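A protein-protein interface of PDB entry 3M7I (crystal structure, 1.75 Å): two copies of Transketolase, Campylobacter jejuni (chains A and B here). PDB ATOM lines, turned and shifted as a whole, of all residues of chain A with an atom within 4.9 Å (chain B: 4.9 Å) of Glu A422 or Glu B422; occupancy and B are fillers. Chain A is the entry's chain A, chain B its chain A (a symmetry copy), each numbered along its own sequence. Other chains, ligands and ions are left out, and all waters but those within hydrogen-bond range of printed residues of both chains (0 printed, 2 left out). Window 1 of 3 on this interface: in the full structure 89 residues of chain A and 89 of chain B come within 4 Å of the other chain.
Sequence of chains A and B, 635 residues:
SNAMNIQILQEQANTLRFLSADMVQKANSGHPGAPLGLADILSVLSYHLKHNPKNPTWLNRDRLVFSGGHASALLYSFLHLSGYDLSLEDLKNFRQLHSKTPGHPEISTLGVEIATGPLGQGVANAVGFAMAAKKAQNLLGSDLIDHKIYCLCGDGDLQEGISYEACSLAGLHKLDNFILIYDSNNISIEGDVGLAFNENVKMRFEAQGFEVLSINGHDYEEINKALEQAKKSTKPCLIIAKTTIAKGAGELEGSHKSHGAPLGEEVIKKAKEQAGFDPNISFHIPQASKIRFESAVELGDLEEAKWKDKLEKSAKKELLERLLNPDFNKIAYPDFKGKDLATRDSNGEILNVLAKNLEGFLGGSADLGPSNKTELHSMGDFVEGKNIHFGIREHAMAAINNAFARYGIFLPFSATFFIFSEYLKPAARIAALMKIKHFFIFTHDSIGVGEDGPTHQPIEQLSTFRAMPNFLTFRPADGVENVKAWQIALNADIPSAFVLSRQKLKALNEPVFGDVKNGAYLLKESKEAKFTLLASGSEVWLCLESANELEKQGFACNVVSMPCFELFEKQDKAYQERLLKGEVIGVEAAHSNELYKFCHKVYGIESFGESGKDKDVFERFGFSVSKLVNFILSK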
ATOM      1  N   PHE A 418      11.330 -37.034  28.740  1.00  0.00           N
ATOM      2  CA  PHE A 418      12.561 -36.288  28.916  1.00  0.00           C
ATOM      3  C   PHE A 418      13.226 -35.912  27.606  1.00  0.00           C
ATOM      4  O   PHE A 418      13.847 -34.817  27.541  1.00  0.00           O
ATOM      5  CB  PHE A 418      13.525 -37.168  29.763  1.00  0.00           C
ATOM      6  CG  PHE A 418      14.784 -36.496  30.280  1.00  0.00           C
ATOM      7  CD1 PHE A 418      14.845 -35.176  30.632  1.00  0.00           C
ATOM      8  CD2 PHE A 418      15.871 -37.299  30.593  1.00  0.00           C
ATOM      9  CE1 PHE A 418      15.976 -34.622  31.162  1.00  0.00           C
ATOM     10  CE2 PHE A 418      16.995 -36.767  31.196  1.00  0.00           C
ATOM     11  CZ  PHE A 418      17.035 -35.431  31.504  1.00  0.00           C
ATOM     12  N   ILE A 419      13.081 -36.749  26.554  1.00  0.00           N
ATOM     13  CA  ILE A 419      13.661 -36.415  25.288  1.00  0.00           C
ATOM     14  C   ILE A 419      13.054 -35.090  24.777  1.00  0.00           C
ATOM     15  O   ILE A 419      13.757 -34.283  24.175  1.00  0.00           O
ATOM     16  CB  ILE A 419      13.575 -37.541  24.223  1.00  0.00           C
ATOM     17  CG1 ILE A 419      14.400 -37.178  22.991  1.00  0.00           C
ATOM     18  CG2 ILE A 419      12.113 -37.847  23.885  1.00  0.00           C
ATOM     19  CD1 ILE A 419      15.799 -36.743  23.188  1.00  0.00           C
ATOM     20  N   PHE A 420      11.770 -34.877  25.008  1.00  0.00           N
ATOM     21  CA  PHE A 420      11.139 -33.653  24.526  1.00  0.00           C
ATOM     22  C   PHE A 420      11.232 -32.475  25.512  1.00  0.00           C
ATOM     23  O   PHE A 420      10.677 -31.408  25.230  1.00  0.00           O
ATOM     24  CB  PHE A 420       9.718 -33.966  24.050  1.00  0.00           C
ATOM     25  CG  PHE A 420       9.659 -35.095  23.050  1.00  0.00           C
ATOM     26  CD1 PHE A 420      10.471 -35.129  21.991  1.00  0.00           C
ATOM     27  CD2 PHE A 420       8.752 -36.130  23.203  1.00  0.00           C
ATOM     28  CE1 PHE A 420      10.453 -36.219  21.024  1.00  0.00           C
ATOM     29  CE2 PHE A 420       8.718 -37.204  22.279  1.00  0.00           C
ATOM     30  CZ  PHE A 420       9.577 -37.230  21.208  1.00  0.00           C
ATOM     31  N   SER A 421      12.098 -32.574  26.551  1.00  0.00           N
ATOM     32  CA  SER A 421      12.473 -31.437  27.354  1.00  0.00           C
ATOM     33  C   SER A 421      13.165 -30.493  26.382  1.00  0.00           C
ATOM     34  O   SER A 421      13.212 -29.305  26.638  1.00  0.00           O
ATOM     35  CB  SER A 421      13.483 -31.849  28.488  1.00  0.00           C
ATOM     36  OG  SER A 421      14.647 -32.415  27.951  1.00  0.00           O
ATOM     37  N   GLU A 422      13.811 -31.000  25.326  1.00  0.00           N
ATOM     38  CA  GLU A 422      14.593 -30.122  24.426  1.00  0.00           C
ATOM     39  C   GLU A 422      13.700 -29.108  23.716  1.00  0.00           C
ATOM     40  O   GLU A 422      14.180 -28.058  23.251  1.00  0.00           O
ATOM     41  CB  GLU A 422      15.390 -30.905  23.414  1.00  0.00           C
ATOM     42  CG  GLU A 422      16.365 -31.876  24.112  1.00  0.00           C
ATOM     43  CD  GLU A 422      17.456 -32.283  23.268  1.00  0.00           C
ATOM     44  OE1 GLU A 422      17.150 -32.499  22.067  1.00  0.00           O
ATOM     45  OE2 GLU A 422      18.618 -32.391  23.790  1.00  0.00           O
ATOM     46  N   TYR A 423      12.437 -29.472  23.530  1.00  0.00           N
ATOM     47  CA  TYR A 423      11.505 -28.528  22.895  1.00  0.00           C
ATOM     48  C   TYR A 423      11.163 -27.333  23.813  1.00  0.00           C
ATOM     49  O   TYR A 423      10.702 -26.313  23.288  1.00  0.00           O
ATOM     50  CB  TYR A 423      10.216 -29.225  22.465  1.00  0.00           C
ATOM     51  CG  TYR A 423      10.197 -29.956  21.171  1.00  0.00           C
ATOM     52  CD1 TYR A 423      10.943 -31.125  20.947  1.00  0.00           C
ATOM     53  CD2 TYR A 423       9.285 -29.587  20.168  1.00  0.00           C
ATOM     54  CE1 TYR A 423      10.925 -31.776  19.758  1.00  0.00           C
ATOM     55  CE2 TYR A 423       9.258 -30.250  18.975  1.00  0.00           C
ATOM     56  CZ  TYR A 423      10.005 -31.374  18.784  1.00  0.00           C
ATOM     57  OH  TYR A 423       9.915 -32.049  17.607  1.00  0.00           O
ATOM     58  N   LEU A 424      11.267 -27.469  25.137  1.00  0.00           N
ATOM     59  CA  LEU A 424      10.856 -26.424  26.114  1.00  0.00           C
ATOM     60  C   LEU A 424      12.046 -25.820  26.865  1.00  0.00           C
ATOM     61  O   LEU A 424      11.857 -24.950  27.684  1.00  0.00           O
ATOM     62  CB  LEU A 424       9.768 -26.967  27.072  1.00  0.00           C
ATOM     63  CG  LEU A 424      10.024 -28.236  27.876  1.00  0.00           C
ATOM     64  CD1 LEU A 424      11.229 -28.032  28.874  1.00  0.00           C
ATOM     65  CD2 LEU A 424       8.794 -28.773  28.675  1.00  0.00           C
ATOM     66  N   LYS A 425      13.253 -26.363  26.635  1.00  0.00           N
ATOM     67  CA  LYS A 425      14.484 -25.909  27.326  1.00  0.00           C
ATOM     68  C   LYS A 425      14.634 -24.353  27.384  1.00  0.00           C
ATOM     69  O   LYS A 425      15.006 -23.846  28.408  1.00  0.00           O
ATOM     70  CB  LYS A 425      15.703 -26.531  26.627  1.00  0.00           C
ATOM     71  CG  LYS A 425      17.079 -25.999  27.133  1.00  0.00           C
ATOM     72  CD  LYS A 425      17.265 -26.301  28.631  1.00  0.00           C
ATOM     73  CE  LYS A 425      18.666 -25.848  29.088  1.00  0.00           C
ATOM     74  NZ  LYS A 425      18.739 -24.298  29.130  1.00  0.00           N
ATOM     75  N   PRO A 426      14.328 -23.602  26.311  1.00  0.00           N
ATOM     76  CA  PRO A 426      14.507 -22.154  26.532  1.00  0.00           C
ATOM     77  C   PRO A 426      13.640 -21.563  27.607  1.00  0.00           C
ATOM     78  O   PRO A 426      14.056 -20.646  28.289  1.00  0.00           O
ATOM     79  CB  PRO A 426      14.258 -21.531  25.117  1.00  0.00           C
ATOM     80  CG  PRO A 426      14.431 -22.682  24.143  1.00  0.00           C
ATOM     81  CD  PRO A 426      13.925 -23.892  24.908  1.00  0.00           C
ATOM     82  N   ARG A 429      14.896 -22.443  30.970  1.00  0.00           N
ATOM     83  CA  ARG A 429      15.994 -21.564  31.337  1.00  0.00           C
ATOM     84  C   ARG A 429      15.512 -20.277  31.996  1.00  0.00           C
ATOM     85  O   ARG A 429      16.099 -19.819  32.909  1.00  0.00           O
ATOM     86  CB  ARG A 429      16.873 -21.238  30.133  1.00  0.00           C
ATOM     87  CG  ARG A 429      18.277 -20.719  30.491  1.00  0.00           C
ATOM     88  CD  ARG A 429      19.171 -20.502  29.272  1.00  0.00           C
ATOM     89  NE  ARG A 429      20.565 -20.369  29.597  1.00  0.00           N
ATOM     90  CZ  ARG A 429      21.229 -19.235  29.638  1.00  0.00           C
ATOM     91  NH1 ARG A 429      20.636 -18.097  29.367  1.00  0.00           N
ATOM     92  NH2 ARG A 429      22.491 -19.254  29.976  1.00  0.00           N
ATOM     93  N   GLU A 460      21.907 -37.152  26.222  1.00  0.00           N
ATOM     94  CA  GLU A 460      22.599 -35.927  26.626  1.00  0.00           C
ATOM     95  C   GLU A 460      21.820 -34.953  27.519  1.00  0.00           C
ATOM     96  O   GLU A 460      22.333 -33.934  27.969  1.00  0.00           O
ATOM     97  CB  GLU A 460      23.169 -35.227  25.390  1.00  0.00           C
ATOM     98  CG  GLU A 460      22.107 -34.461  24.478  1.00  0.00           C
ATOM     99  CD  GLU A 460      21.354 -35.384  23.454  1.00  0.00           C
ATOM    100  OE1 GLU A 460      21.203 -36.593  23.690  1.00  0.00           O
ATOM    101  OE2 GLU A 460      20.814 -34.878  22.415  1.00  0.00           O
ATOM    102  N   GLN A 461      20.517 -35.197  27.695  1.00  0.00           N
ATOM    103  CA  GLN A 461      19.663 -34.319  28.473  1.00  0.00           C
ATOM    104  C   GLN A 461      20.019 -34.160  29.963  1.00  0.00           C
ATOM    105  O   GLN A 461      19.907 -33.050  30.478  1.00  0.00           O
ATOM    106  CB  GLN A 461      18.157 -34.682  28.228  1.00  0.00           C
ATOM    107  CG  GLN A 461      17.781 -34.411  26.790  1.00  0.00           C
ATOM    108  CD  GLN A 461      18.315 -35.425  25.792  1.00  0.00           C
ATOM    109  OE1 GLN A 461      18.575 -36.588  26.119  1.00  0.00           O
ATOM    110  NE2 GLN A 461      18.504 -34.991  24.565  1.00  0.00           N
ATOM    111  N   PHE B 418      24.531 -18.444  19.975  1.00  0.00           N
ATOM    112  CA  PHE B 418      24.619 -19.736  20.627  1.00  0.00           C
ATOM    113  C   PHE B 418      23.554 -19.947  21.686  1.00  0.00           C
ATOM    114  O   PHE B 418      23.095 -21.109  21.853  1.00  0.00           O
ATOM    115  CB  PHE B 418      26.032 -19.841  21.271  1.00  0.00           C
ATOM    116  CG  PHE B 418      26.440 -21.204  21.801  1.00  0.00           C
ATOM    117  CD1 PHE B 418      26.040 -22.383  21.236  1.00  0.00           C
ATOM    118  CD2 PHE B 418      27.418 -21.256  22.782  1.00  0.00           C
ATOM    119  CE1 PHE B 418      26.486 -23.591  21.695  1.00  0.00           C
ATOM    120  CE2 PHE B 418      27.932 -22.467  23.207  1.00  0.00           C
ATOM    121  CZ  PHE B 418      27.483 -23.633  22.643  1.00  0.00           C
ATOM    122  N   ILE B 419      23.114 -18.867  22.371  1.00  0.00           N
ATOM    123  CA  ILE B 419      22.083 -19.015  23.354  1.00  0.00           C
ATOM    124  C   ILE B 419      20.803 -19.558  22.682  1.00  0.00           C
ATOM    125  O   ILE B 419      20.089 -20.360  23.276  1.00  0.00           O
ATOM    126  CB  ILE B 419      21.802 -17.736  24.188  1.00  0.00           C
ATOM    127  CG1 ILE B 419      20.851 -18.047  25.342  1.00  0.00           C
ATOM    128  CG2 ILE B 419      21.287 -16.611  23.286  1.00  0.00           C
ATOM    129  CD1 ILE B 419      21.167 -19.193  26.221  1.00  0.00           C
ATOM    130  N   PHE B 420      20.519 -19.121  21.467  1.00  0.00           N
ATOM    131  CA  PHE B 420      19.310 -19.583  20.794  1.00  0.00           C
ATOM    132  C   PHE B 420      19.502 -20.879  19.987  1.00  0.00           C
ATOM    133  O   PHE B 420      18.558 -21.324  19.328  1.00  0.00           O
ATOM    134  CB  PHE B 420      18.700 -18.428  19.996  1.00  0.00           C
ATOM    135  CG  PHE B 420      18.479 -17.184  20.820  1.00  0.00           C
ATOM    136  CD1 PHE B 420      17.874 -17.235  22.008  1.00  0.00           C
ATOM    137  CD2 PHE B 420      18.897 -15.946  20.360  1.00  0.00           C
ATOM    138  CE1 PHE B 420      17.670 -16.054  22.837  1.00  0.00           C
ATOM    139  CE2 PHE B 420      18.716 -14.782  21.150  1.00  0.00           C
ATOM    140  CZ  PHE B 420      18.110 -14.861  22.379  1.00  0.00           C
ATOM    141  N   SER B 421      20.628 -21.605  20.198  1.00  0.00           N
ATOM    142  CA  SER B 421      20.774 -22.957  19.722  1.00  0.00           C
ATOM    143  C   SER B 421      19.687 -23.739  20.446  1.00  0.00           C
ATOM    144  O   SER B 421      19.277 -24.776  19.962  1.00  0.00           O
ATOM    145  CB  SER B 421      22.182 -23.548  20.105  1.00  0.00           C
ATOM    146  OG  SER B 421      22.375 -23.544  21.492  1.00  0.00           O
ATOM    147  N   GLU B 422      19.289 -23.334  21.657  1.00  0.00           N
ATOM    148  CA  GLU B 422      18.320 -24.134  22.440  1.00  0.00           C
ATOM    149  C   GLU B 422      16.966 -24.217  21.740  1.00  0.00           C
ATOM    150  O   GLU B 422      16.171 -25.137  22.007  1.00  0.00           O
ATOM    151  CB  GLU B 422      18.145 -23.609  23.842  1.00  0.00           C
ATOM    152  CG  GLU B 422      19.489 -23.599  24.599  1.00  0.00           C
ATOM    153  CD  GLU B 422      19.330 -23.578  26.028  1.00  0.00           C
ATOM    154  OE1 GLU B 422      18.397 -22.849  26.452  1.00  0.00           O
ATOM    155  OE2 GLU B 422      20.130 -24.282  26.736  1.00  0.00           O
ATOM    156  N   TYR B 423      16.659 -23.203  20.941  1.00  0.00           N
ATOM    157  CA  TYR B 423      15.391 -23.236  20.196  1.00  0.00           C
ATOM    158  C   TYR B 423      15.399 -24.293  19.068  1.00  0.00           C
ATOM    159  O   TYR B 423      14.311 -24.670  18.621  1.00  0.00           O
ATOM    160  CB  TYR B 423      15.057 -21.866  19.608  1.00  0.00           C
ATOM    161  CG  TYR B 423      14.402 -20.856  20.478  1.00  0.00           C
ATOM    162  CD1 TYR B 423      15.048 -20.264  21.576  1.00  0.00           C
ATOM    163  CD2 TYR B 423      13.149 -20.328  20.124  1.00  0.00           C
ATOM    164  CE1 TYR B 423      14.435 -19.351  22.369  1.00  0.00           C
ATOM    165  CE2 TYR B 423      12.536 -19.400  20.915  1.00  0.00           C
ATOM    166  CZ  TYR B 423      13.186 -18.854  21.982  1.00  0.00           C
ATOM    167  OH  TYR B 423      12.574 -17.889  22.719  1.00  0.00           O
ATOM    168  N   LEU B 424      16.562 -24.681  18.539  1.00  0.00           N
ATOM    169  CA  LEU B 424      16.677 -25.604  17.377  1.00  0.00           C
ATOM    170  C   LEU B 424      17.291 -26.955  17.757  1.00  0.00           C
ATOM    171  O   LEU B 424      17.434 -27.806  16.909  1.00  0.00           O
ATOM    172  CB  LEU B 424      17.431 -24.922  16.209  1.00  0.00           C
ATOM    173  CG  LEU B 424      18.818 -24.334  16.435  1.00  0.00           C
ATOM    174  CD1 LEU B 424      19.846 -25.462  16.838  1.00  0.00           C
ATOM    175  CD2 LEU B 424      19.401 -23.529  15.231  1.00  0.00           C
ATOM    176  N   LYS B 425      17.729 -27.093  19.019  1.00  0.00           N
ATOM    177  CA  LYS B 425      18.384 -28.329  19.512  1.00  0.00           C
ATOM    178  C   LYS B 425      17.649 -29.642  19.087  1.00  0.00           C
ATOM    179  O   LYS B 425      18.305 -30.575  18.708  1.00  0.00           O
ATOM    180  CB  LYS B 425      18.492 -28.257  21.043  1.00  0.00           C
ATOM    181  CG  LYS B 425      18.998 -29.568  21.717  1.00  0.00           C
ATOM    182  CD  LYS B 425      20.410 -29.929  21.223  1.00  0.00           C
ATOM    183  CE  LYS B 425      20.926 -31.175  21.968  1.00  0.00           C
ATOM    184  NZ  LYS B 425      20.159 -32.438  21.491  1.00  0.00           N
ATOM    185  N   PRO B 426      16.306 -29.710  19.125  1.00  0.00           N
ATOM    186  CA  PRO B 426      15.766 -31.009  18.678  1.00  0.00           C
ATOM    187  C   PRO B 426      16.075 -31.368  17.251  1.00  0.00           C
ATOM    188  O   PRO B 426      16.251 -32.531  16.942  1.00  0.00           O
ATOM    189  CB  PRO B 426      14.233 -30.893  18.975  1.00  0.00           C
ATOM    190  CG  PRO B 426      14.110 -29.763  19.980  1.00  0.00           C
ATOM    191  CD  PRO B 426      15.223 -28.805  19.595  1.00  0.00           C
ATOM    192  N   ARG B 429      19.585 -32.463  16.880  1.00  0.00           N
ATOM    193  CA  ARG B 429      19.718 -33.852  17.285  1.00  0.00           C
ATOM    194  C   ARG B 429      19.432 -34.821  16.144  1.00  0.00           C
ATOM    195  O   ARG B 429      20.085 -35.792  16.009  1.00  0.00           O
ATOM    196  CB  ARG B 429      18.825 -34.172  18.480  1.00  0.00           C
ATOM    197  CG  ARG B 429      19.228 -35.439  19.255  1.00  0.00           C
ATOM    198  CD  ARG B 429      18.384 -35.678  20.506  1.00  0.00           C
ATOM    199  NE  ARG B 429      18.961 -36.627  21.417  1.00  0.00           N
ATOM    200  CZ  ARG B 429      18.578 -37.878  21.553  1.00  0.00           C
ATOM    201  NH1 ARG B 429      17.594 -38.362  20.835  1.00  0.00           N
ATOM    202  NH2 ARG B 429      19.210 -38.643  22.403  1.00  0.00           N
ATOM    203  N   GLU B 460      25.513 -23.115  29.745  1.00  0.00           N
ATOM    204  CA  GLU B 460      25.380 -24.572  29.692  1.00  0.00           C
ATOM    205  C   GLU B 460      25.364 -25.216  28.300  1.00  0.00           C
ATOM    206  O   GLU B 460      25.328 -26.433  28.149  1.00  0.00           O
ATOM    207  CB  GLU B 460      24.176 -25.009  30.531  1.00  0.00           C
ATOM    208  CG  GLU B 460      22.746 -24.742  29.879  1.00  0.00           C
ATOM    209  CD  GLU B 460      22.204 -23.283  30.090  1.00  0.00           C
ATOM    210  OE1 GLU B 460      22.991 -22.337  30.254  1.00  0.00           O
ATOM    211  OE2 GLU B 460      20.954 -23.046  30.006  1.00  0.00           O
ATOM    212  N   GLN B 461      25.272 -24.395  27.250  1.00  0.00           N
ATOM    213  CA  GLN B 461      25.194 -24.886  25.886  1.00  0.00           C
ATOM    214  C   GLN B 461      26.403 -25.694  25.379  1.00  0.00           C
ATOM    215  O   GLN B 461      26.197 -26.672  24.664  1.00  0.00           O
ATOM    216  CB  GLN B 461      24.771 -23.724  24.921  1.00  0.00           C
ATOM    217  CG  GLN B 461      23.371 -23.259  25.244  1.00  0.00           C
ATOM    218  CD  GLN B 461      23.255 -22.419  26.506  1.00  0.00           C
ATOM    219  OE1 GLN B 461      24.206 -21.757  26.938  1.00  0.00           O
ATOM    220  NE2 GLN B 461      22.095 -22.450  27.123  1.00  0.00           N
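Of chain B, only Glu B422 (3.7 Å), Lys B425 (2.8 Å), Pro B426 (3.7 Å) and Arg B429 (3.8 Å) come within 4 Å of Glu A422. Of the printed residues of chain B, Lys A425 touches Glu B422 and Glu B460. Printed residues of chain B within 4 Å of Arg A429: Ile B419 (3.4 Å), Glu B422 (3.7 Å), Glu B460 (2.7 Å) and Gln B461 (3.6 Å). Glu B422 touches four residues of chain A. The nearest printed residue of chain A that does not touch Glu B422 is Tyr A423 (5.7 Å). The nearest printed residue of chain B that does not touch Ile A419 is Pro B426 (6.2 Å).
The side-chain amino group (NZ) of Lys B425 is in salt-bridge range of the side-chain carboxylate (OE2) of Glu A422 (2.8 Å). The side-chain carboxylate (OE2) of Glu B422 lies within salt-bridge range of the side-chain amino group (NZ) of Lys A425 (2.8 Å). The side-chain amino group (NZ) of Lys A425 is in salt-bridge range of the side-chain carboxylate (OE2) of Glu B460, at 2.7 Å. The guanidinium group (NE) of Arg A429 is in salt-bridge range of the side-chain carboxylate (OE2) of Glu B460 (2.7 Å). The side-chain carboxylate (OE2) of Glu A460 lies within salt-bridge range of the side-chain amino group (NZ) of Lys B425 (2.7 Å). The side-chain carboxylate (OE2) of Glu A460 is in salt-bridge range of the guanidinium group (NE) of Arg B429, 2.7 Å away.
Printed residues of chain A that touch a printed residue of chain B: Ile A419, Glu A422, Tyr A423, Lys A425, Pro A426, Arg A429, Glu A460 and Gln A461. Hydrophobic or aromatic side chains of chain A within 4 Å of the printed part of chain B: Ile A419, Tyr A423 and Pro A426. Along chain A the printed residues that touch a printed residue of chain B span positions 419 to 461. Of the 12 printed residues of chain B, 8 touch a printed residue of chain A. Among the printed residues, Asp or Glu carboxylates within 4 Å of a Lys or Arg side-chain nitrogen of the other chain: Glu A422 with Lys B425, Lys A425 with Glu B422, Lys A425 with Glu B460, Arg A429 with Glu B460, Glu A460 with Lys B425 and Glu A460 with Arg B429.
The side-chain amide nitrogen (NE2) of Gln A461 lies within hydrogen-bond range of the side-chain carboxylate (OE2) of Glu A422, 2.7 Å away. OE2 of Glu A460 sits close to NE2 of Gln A461 (3.2 Å). The side-chain amide nitrogen of Gln B461 lies within hydrogen-bond range of the side-chain carboxylate of Glu B422 (2.7 Å). OE2 of Glu B460 sits close to NE2 of Gln B461 (3.2 Å).
Among the printed residues, merely in contact across the chains: Ile A419 with Arg B429, Glu A422 with Glu B422, Glu A422 with Pro B426, Glu A422 with Arg B429, Tyr A423 with Pro B426, Pro A426 with Glu B422, Pro A426 with Tyr B423, Arg A429 with Ile B419, Arg A429 with Glu B422, Arg A429 with Gln B461 and Gln A461 with Arg B429.
Glu A422 touches its own counterpart, Glu B422. Tyr A423 touches Pro B426, and with the chains exchanged Pro A426 touches Tyr B423. Lys A425 touches Glu B460, and with the chains exchanged Glu A460 touches Lys B425. Arg A429 touches Gln B461, and with the chains exchanged Gln A461 touches Arg B429. 12 positions are printed for both chains. Of the 17 pairs that touch across the chains among the printed residues, 17 have their exchanged pair printed and touching as well.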
